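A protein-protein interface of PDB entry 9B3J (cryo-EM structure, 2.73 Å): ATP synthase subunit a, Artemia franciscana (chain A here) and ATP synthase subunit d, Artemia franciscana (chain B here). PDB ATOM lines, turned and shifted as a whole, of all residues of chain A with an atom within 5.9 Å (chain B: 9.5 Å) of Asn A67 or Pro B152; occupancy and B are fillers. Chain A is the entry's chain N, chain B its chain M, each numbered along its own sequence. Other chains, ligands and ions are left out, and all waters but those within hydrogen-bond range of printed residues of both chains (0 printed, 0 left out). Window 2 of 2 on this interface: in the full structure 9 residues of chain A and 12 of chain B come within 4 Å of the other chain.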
ATOM      1  N   ASN A  52      19.350 -12.803  18.116  1.00  0.00           N
ATOM      2  CA  ASN A  52      19.232 -13.172  19.520  1.00  0.00           C
ATOM      3  C   ASN A  52      19.916 -12.151  20.414  1.00  0.00           C
ATOM      4  O   ASN A  52      19.386 -11.785  21.471  1.00  0.00           O
ATOM      5  CB  ASN A  52      19.817 -14.563  19.743  1.00  0.00           C
ATOM      6  CG  ASN A  52      20.010 -14.881  21.201  1.00  0.00           C
ATOM      7  OD1 ASN A  52      19.048 -15.105  21.930  1.00  0.00           O
ATOM      8  ND2 ASN A  52      21.259 -14.908  21.637  1.00  0.00           N
ATOM      9  N   SER A  56      17.898  -9.839  23.111  1.00  0.00           N
ATOM     10  CA  SER A  56      18.216  -9.990  24.525  1.00  0.00           C
ATOM     11  C   SER A  56      18.251  -8.649  25.245  1.00  0.00           C
ATOM     12  O   SER A  56      18.000  -8.594  26.453  1.00  0.00           O
ATOM     13  CB  SER A  56      19.553 -10.706  24.687  1.00  0.00           C
ATOM     14  OG  SER A  56      20.619  -9.886  24.244  1.00  0.00           O
ATOM     15  N   MET A  59      14.611  -8.018  26.002  1.00  0.00           N
ATOM     16  CA  MET A  59      13.913  -9.071  26.735  1.00  0.00           C
ATOM     17  C   MET A  59      14.077  -8.922  28.243  1.00  0.00           C
ATOM     18  O   MET A  59      13.097  -8.734  28.970  1.00  0.00           O
ATOM     19  CB  MET A  59      14.417 -10.439  26.279  1.00  0.00           C
ATOM     20  CG  MET A  59      13.599 -11.065  25.172  1.00  0.00           C
ATOM     21  SD  MET A  59      14.510 -12.379  24.347  1.00  0.00           S
ATOM     22  CE  MET A  59      15.153 -13.269  25.760  1.00  0.00           C
ATOM     23  N   SER A  63      13.011 -13.617  31.247  1.00  0.00           N
ATOM     24  CA  SER A  63      12.379 -14.068  30.015  1.00  0.00           C
ATOM     25  C   SER A  63      13.253 -15.107  29.330  1.00  0.00           C
ATOM     26  O   SER A  63      13.632 -14.962  28.167  1.00  0.00           O
ATOM     27  CB  SER A  63      12.100 -12.886  29.097  1.00  0.00           C
ATOM     28  OG  SER A  63      13.285 -12.152  28.857  1.00  0.00           O
ATOM     29  N   PHE A  64      13.635 -16.146  30.085  1.00  0.00           N
ATOM     30  CA  PHE A  64      14.519 -17.189  29.564  1.00  0.00           C
ATOM     31  C   PHE A  64      13.924 -17.899  28.355  1.00  0.00           C
ATOM     32  O   PHE A  64      14.660 -18.286  27.442  1.00  0.00           O
ATOM     33  CB  PHE A  64      14.838 -18.198  30.668  1.00  0.00           C
ATOM     34  CG  PHE A  64      15.428 -19.494  30.169  1.00  0.00           C
ATOM     35  CD1 PHE A  64      16.702 -19.537  29.626  1.00  0.00           C
ATOM     36  CD2 PHE A  64      14.711 -20.675  30.261  1.00  0.00           C
ATOM     37  CE1 PHE A  64      17.237 -20.733  29.176  1.00  0.00           C
ATOM     38  CE2 PHE A  64      15.247 -21.870  29.813  1.00  0.00           C
ATOM     39  CZ  PHE A  64      16.507 -21.897  29.273  1.00  0.00           C
ATOM     40  N   GLY A  65      12.605 -18.058  28.315  1.00  0.00           N
ATOM     41  CA  GLY A  65      11.988 -18.715  27.179  1.00  0.00           C
ATOM     42  C   GLY A  65      11.835 -17.867  25.939  1.00  0.00           C
ATOM     43  O   GLY A  65      11.539 -18.410  24.871  1.00  0.00           O
ATOM     44  N   ALA A  66      12.042 -16.557  26.039  1.00  0.00           N
ATOM     45  CA  ALA A  66      11.832 -15.668  24.906  1.00  0.00           C
ATOM     46  C   ALA A  66      13.023 -15.614  23.966  1.00  0.00           C
ATOM     47  O   ALA A  66      12.972 -14.878  22.976  1.00  0.00           O
ATOM     48  CB  ALA A  66      11.504 -14.257  25.391  1.00  0.00           C
ATOM     49  N   ASN A  67      14.097 -16.346  24.261  1.00  0.00           N
ATOM     50  CA  ASN A  67      15.221 -16.403  23.334  1.00  0.00           C
ATOM     51  C   ASN A  67      14.845 -17.142  22.060  1.00  0.00           C
ATOM     52  O   ASN A  67      15.155 -16.687  20.956  1.00  0.00           O
ATOM     53  CB  ASN A  67      16.416 -17.074  23.998  1.00  0.00           C
ATOM     54  CG  ASN A  67      16.975 -16.265  25.136  1.00  0.00           C
ATOM     55  OD1 ASN A  67      16.597 -16.453  26.292  1.00  0.00           O
ATOM     56  ND2 ASN A  67      17.885 -15.353  24.819  1.00  0.00           N
ATOM     57  N   ILE A  68      14.157 -18.272  22.192  1.00  0.00           N
ATOM     58  CA  ILE A  68      13.876 -19.135  21.054  1.00  0.00           C
ATOM     59  C   ILE A  68      12.435 -19.014  20.577  1.00  0.00           C
ATOM     60  O   ILE A  68      12.159 -19.290  19.400  1.00  0.00           O
ATOM     61  CB  ILE A  68      14.222 -20.596  21.413  1.00  0.00           C
ATOM     62  CG1 ILE A  68      14.325 -21.481  20.183  1.00  0.00           C
ATOM     63  CG2 ILE A  68      13.219 -21.181  22.384  1.00  0.00           C
ATOM     64  CD1 ILE A  68      14.805 -22.850  20.522  1.00  0.00           C
ATOM     65  N   LEU A  69      11.520 -18.565  21.434  1.00  0.00           N
ATOM     66  CA  LEU A  69      10.107 -18.521  21.091  1.00  0.00           C
ATOM     67  C   LEU A  69       9.795 -17.445  20.065  1.00  0.00           C
ATOM     68  O   LEU A  69       8.775 -17.537  19.377  1.00  0.00           O
ATOM     69  CB  LEU A  69       9.286 -18.284  22.354  1.00  0.00           C
ATOM     70  CG  LEU A  69       7.820 -18.684  22.332  1.00  0.00           C
ATOM     71  CD1 LEU A  69       7.701 -20.155  22.635  1.00  0.00           C
ATOM     72  CD2 LEU A  69       7.038 -17.851  23.328  1.00  0.00           C
ATOM     73  N   VAL A  70      10.644 -16.430  19.952  1.00  0.00           N
ATOM     74  CA  VAL A  70      10.417 -15.344  19.013  1.00  0.00           C
ATOM     75  C   VAL A  70      11.303 -15.553  17.797  1.00  0.00           C
ATOM     76  O   VAL A  70      11.003 -15.062  16.705  1.00  0.00           O
ATOM     77  CB  VAL A  70      10.693 -13.981  19.660  1.00  0.00           C
ATOM     78  CG1 VAL A  70       9.896 -12.927  18.969  1.00  0.00           C
ATOM     79  CG2 VAL A  70      10.329 -14.016  21.114  1.00  0.00           C
ATOM     80  N   ILE A  71      12.411 -16.270  17.980  1.00  0.00           N
ATOM     81  CA  ILE A  71      13.269 -16.586  16.845  1.00  0.00           C
ATOM     82  C   ILE A  71      12.584 -17.586  15.925  1.00  0.00           C
ATOM     83  O   ILE A  71      12.615 -17.440  14.696  1.00  0.00           O
ATOM     84  CB  ILE A  71      14.639 -17.081  17.337  1.00  0.00           C
ATOM     85  CG1 ILE A  71      15.501 -15.876  17.705  1.00  0.00           C
ATOM     86  CG2 ILE A  71      15.332 -17.934  16.296  1.00  0.00           C
ATOM     87  CD1 ILE A  71      16.899 -16.220  18.117  1.00  0.00           C
ATOM     88  N   ALA A  72      11.922 -18.589  16.499  1.00  0.00           N
ATOM     89  CA  ALA A  72      11.185 -19.547  15.683  1.00  0.00           C
ATOM     90  C   ALA A  72      10.026 -18.880  14.956  1.00  0.00           C
ATOM     91  O   ALA A  72       9.725 -19.222  13.808  1.00  0.00           O
ATOM     92  CB  ALA A  72      10.680 -20.694  16.548  1.00  0.00           C
ATOM     93  N   VAL B 144      24.689 -31.819  25.195  1.00  0.00           N
ATOM     94  CA  VAL B 144      23.530 -31.078  25.674  1.00  0.00           C
ATOM     95  C   VAL B 144      22.385 -32.079  25.777  1.00  0.00           C
ATOM     96  O   VAL B 144      22.030 -32.738  24.794  1.00  0.00           O
ATOM     97  CB  VAL B 144      23.193 -29.881  24.762  1.00  0.00           C
ATOM     98  CG1 VAL B 144      23.378 -30.232  23.289  1.00  0.00           C
ATOM     99  CG2 VAL B 144      21.785 -29.382  25.034  1.00  0.00           C
ATOM    100  N   PRO B 149      20.408 -27.696  31.699  1.00  0.00           N
ATOM    101  CA  PRO B 149      20.059 -26.295  31.438  1.00  0.00           C
ATOM    102  C   PRO B 149      20.141 -25.963  29.959  1.00  0.00           C
ATOM    103  O   PRO B 149      21.216 -26.034  29.346  1.00  0.00           O
ATOM    104  CB  PRO B 149      21.112 -25.522  32.242  1.00  0.00           C
ATOM    105  CG  PRO B 149      21.369 -26.396  33.400  1.00  0.00           C
ATOM    106  CD  PRO B 149      21.267 -27.816  32.891  1.00  0.00           C
ATOM    107  N   PRO B 150      19.020 -25.590  29.358  1.00  0.00           N
ATOM    108  CA  PRO B 150      18.978 -25.405  27.907  1.00  0.00           C
ATOM    109  C   PRO B 150      19.192 -23.969  27.463  1.00  0.00           C
ATOM    110  O   PRO B 150      19.275 -23.058  28.292  1.00  0.00           O
ATOM    111  CB  PRO B 150      17.566 -25.883  27.556  1.00  0.00           C
ATOM    112  CG  PRO B 150      16.751 -25.695  28.855  1.00  0.00           C
ATOM    113  CD  PRO B 150      17.701 -25.363  29.970  1.00  0.00           C
ATOM    114  N   SER B 151      19.289 -23.776  26.141  1.00  0.00           N
ATOM    115  CA  SER B 151      19.295 -22.495  25.437  1.00  0.00           C
ATOM    116  C   SER B 151      19.241 -22.745  23.932  1.00  0.00           C
ATOM    117  O   SER B 151      19.694 -23.797  23.470  1.00  0.00           O
ATOM    118  CB  SER B 151      20.533 -21.673  25.788  1.00  0.00           C
ATOM    119  OG  SER B 151      20.476 -21.264  27.142  1.00  0.00           O
ATOM    120  N   PRO B 152      18.671 -21.828  23.141  1.00  0.00           N
ATOM    121  CA  PRO B 152      18.784 -21.962  21.679  1.00  0.00           C
ATOM    122  C   PRO B 152      20.204 -21.815  21.187  1.00  0.00           C
ATOM    123  O   PRO B 152      20.557 -22.385  20.148  1.00  0.00           O
ATOM    124  CB  PRO B 152      17.898 -20.830  21.154  1.00  0.00           C
ATOM    125  CG  PRO B 152      17.922 -19.827  22.238  1.00  0.00           C
ATOM    126  CD  PRO B 152      17.945 -20.608  23.519  1.00  0.00           C
ATOM    127  N   ASN B 153      21.007 -21.024  21.889  1.00  0.00           N
ATOM    128  CA  ASN B 153      22.450 -20.943  21.713  1.00  0.00           C
ATOM    129  C   ASN B 153      23.038 -21.620  22.937  1.00  0.00           C
ATOM    130  O   ASN B 153      23.254 -20.982  23.967  1.00  0.00           O
ATOM    131  CB  ASN B 153      22.915 -19.510  21.596  1.00  0.00           C
ATOM    132  CG  ASN B 153      22.069 -18.557  22.409  1.00  0.00           C
ATOM    133  OD1 ASN B 153      21.471 -17.628  21.870  1.00  0.00           O
ATOM    134  ND2 ASN B 153      22.007 -18.784  23.714  1.00  0.00           N
ATOM    135  N   VAL B 154      23.289 -22.919  22.826  1.00  0.00           N
ATOM    136  CA  VAL B 154      23.725 -23.678  23.986  1.00  0.00           C
ATOM    137  C   VAL B 154      25.174 -23.297  24.236  1.00  0.00           C
ATOM    138  O   VAL B 154      26.097 -23.896  23.675  1.00  0.00           O
ATOM    139  CB  VAL B 154      23.560 -25.191  23.765  1.00  0.00           C
ATOM    140  CG1 VAL B 154      23.420 -25.898  25.091  1.00  0.00           C
ATOM    141  CG2 VAL B 154      22.363 -25.474  22.890  1.00  0.00           C
ATOM    142  N   LYS B 155      25.375 -22.307  25.092  1.00  0.00           N
ATOM    143  CA  LYS B 155      26.651 -21.644  25.266  1.00  0.00           C
ATOM    144  C   LYS B 155      27.195 -21.943  26.659  1.00  0.00           C
ATOM    145  O   LYS B 155      26.629 -22.745  27.412  1.00  0.00           O
ATOM    146  CB  LYS B 155      26.486 -20.142  25.031  1.00  0.00           C
ATOM    147  CG  LYS B 155      27.624 -19.491  24.279  1.00  0.00           C
ATOM    148  CD  LYS B 155      27.710 -18.014  24.615  1.00  0.00           C
ATOM    149  CE  LYS B 155      26.401 -17.306  24.338  1.00  0.00           C
ATOM    150  NZ  LYS B 155      26.054 -17.361  22.896  1.00  0.00           N
ATOM    151  N   LYS B 157      27.569 -19.441  28.903  1.00  0.00           N
ATOM    152  CA  LYS B 157      26.843 -18.621  29.869  1.00  0.00           C
ATOM    153  C   LYS B 157      25.478 -18.097  29.412  1.00  0.00           C
ATOM    154  O   LYS B 157      25.234 -16.889  29.531  1.00  0.00           O
ATOM    155  CB  LYS B 157      27.721 -17.433  30.270  1.00  0.00           C
ATOM    156  CG  LYS B 157      28.422 -16.746  29.102  1.00  0.00           C
ATOM    157  CD  LYS B 157      29.909 -17.056  29.076  1.00  0.00           C
ATOM    158  CE  LYS B 157      30.613 -16.491  30.298  1.00  0.00           C
ATOM    159  NZ  LYS B 157      30.503 -15.009  30.364  1.00  0.00           N
ATOM    160  N   PRO B 158      24.536 -18.934  28.906  1.00  0.00           N
ATOM    161  CA  PRO B 158      23.194 -18.398  28.645  1.00  0.00           C
ATOM    162  C   PRO B 158      22.172 -18.709  29.733  1.00  0.00           C
ATOM    163  O   PRO B 158      21.056 -18.181  29.694  1.00  0.00           O
ATOM    164  CB  PRO B 158      22.816 -19.064  27.319  1.00  0.00           C
ATOM    165  CG  PRO B 158      23.589 -20.351  27.306  1.00  0.00           C
ATOM    166  CD  PRO B 158      24.624 -20.316  28.397  1.00  0.00           C
ATOM    167  N   PHE B 159      22.525 -19.548  30.703  1.00  0.00           N
ATOM    168  CA  PHE B 159      21.602 -19.976  31.740  1.00  0.00           C
ATOM    169  C   PHE B 159      22.154 -19.626  33.114  1.00  0.00           C
ATOM    170  O   PHE B 159      23.368 -19.505  33.304  1.00  0.00           O
ATOM    171  CB  PHE B 159      21.321 -21.485  31.663  1.00  0.00           C
ATOM    172  CG  PHE B 159      22.550 -22.331  31.513  1.00  0.00           C
ATOM    173  CD1 PHE B 159      23.307 -22.693  32.615  1.00  0.00           C
ATOM    174  CD2 PHE B 159      22.933 -22.790  30.267  1.00  0.00           C
ATOM    175  CE1 PHE B 159      24.430 -23.474  32.474  1.00  0.00           C
ATOM    176  CE2 PHE B 159      24.057 -23.572  30.120  1.00  0.00           C
ATOM    177  CZ  PHE B 159      24.806 -23.916  31.225  1.00  0.00           C
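Phe A64 touches Pro B150 (CZ to O, 3.2 Å). Phe A64 touches Ser B151 (CE1 to OG, 3.9 Å). CB of Asn A67 touches CG of Pro B152 (3.6 Å). Ile A68 touches Pro B152 (CB to CB, 3.7 Å).
ND2 of Asn A67 sits at hydrogen-bond distance from OD1 of Asn A52 (3.1 Å). The backbone carbonyl oxygen (O) of Phe A64 sits close to the side-chain amide oxygen (OD1) of Asn A67 (2.9 Å).
The side-chain amide nitrogen (ND2) of Asn A52 is in hydrogen-bond range of the side-chain amide oxygen (OD1) of Asn B153, at 2.7 Å.
Printed residues of chain B that touch a printed residue of chain A: Pro B150, Ser B151, Pro B152 and Asn B153. Hydrophobic or aromatic side chains of chain B within 4 Å of the printed part of chain A: Pro B150 and Pro B152. Among the printed residues, 5 pairs touch across the chains. Among the printed residues, no Asp or Glu carboxylate lies within 4 Å of a Lys or Arg side-chain nitrogen of the other chain.
Printed residues of chain B within 4 Å of Asn A52: Asn B153 (2.7 Å). Printed residues of chain B within 4 Å of Phe A64: Pro B150 (3.2 Å) and Ser B151 (3.9 Å). No residue of chain B comes within 4 Å of Gly A65. Ala A66 touches none of the printed residues of chain B. Ile A68 touches just one residue of chain B: Pro B152. Of the printed residues of chain A, Pro B150 touches Phe A64 (3.2 Å). Printed residues of chain A within 4 Å of Ser B151: Phe A64 (3.9 Å). Of chain A, only Asn A67 and Ile A68 come within 4 Å of Pro B152. Of the printed residues of chain A, Asn B153 touches Asn A52 (2.7 Å). The nearest residue of chain A that does not touch Pro B152 is Asn A52 (4.9 Å).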
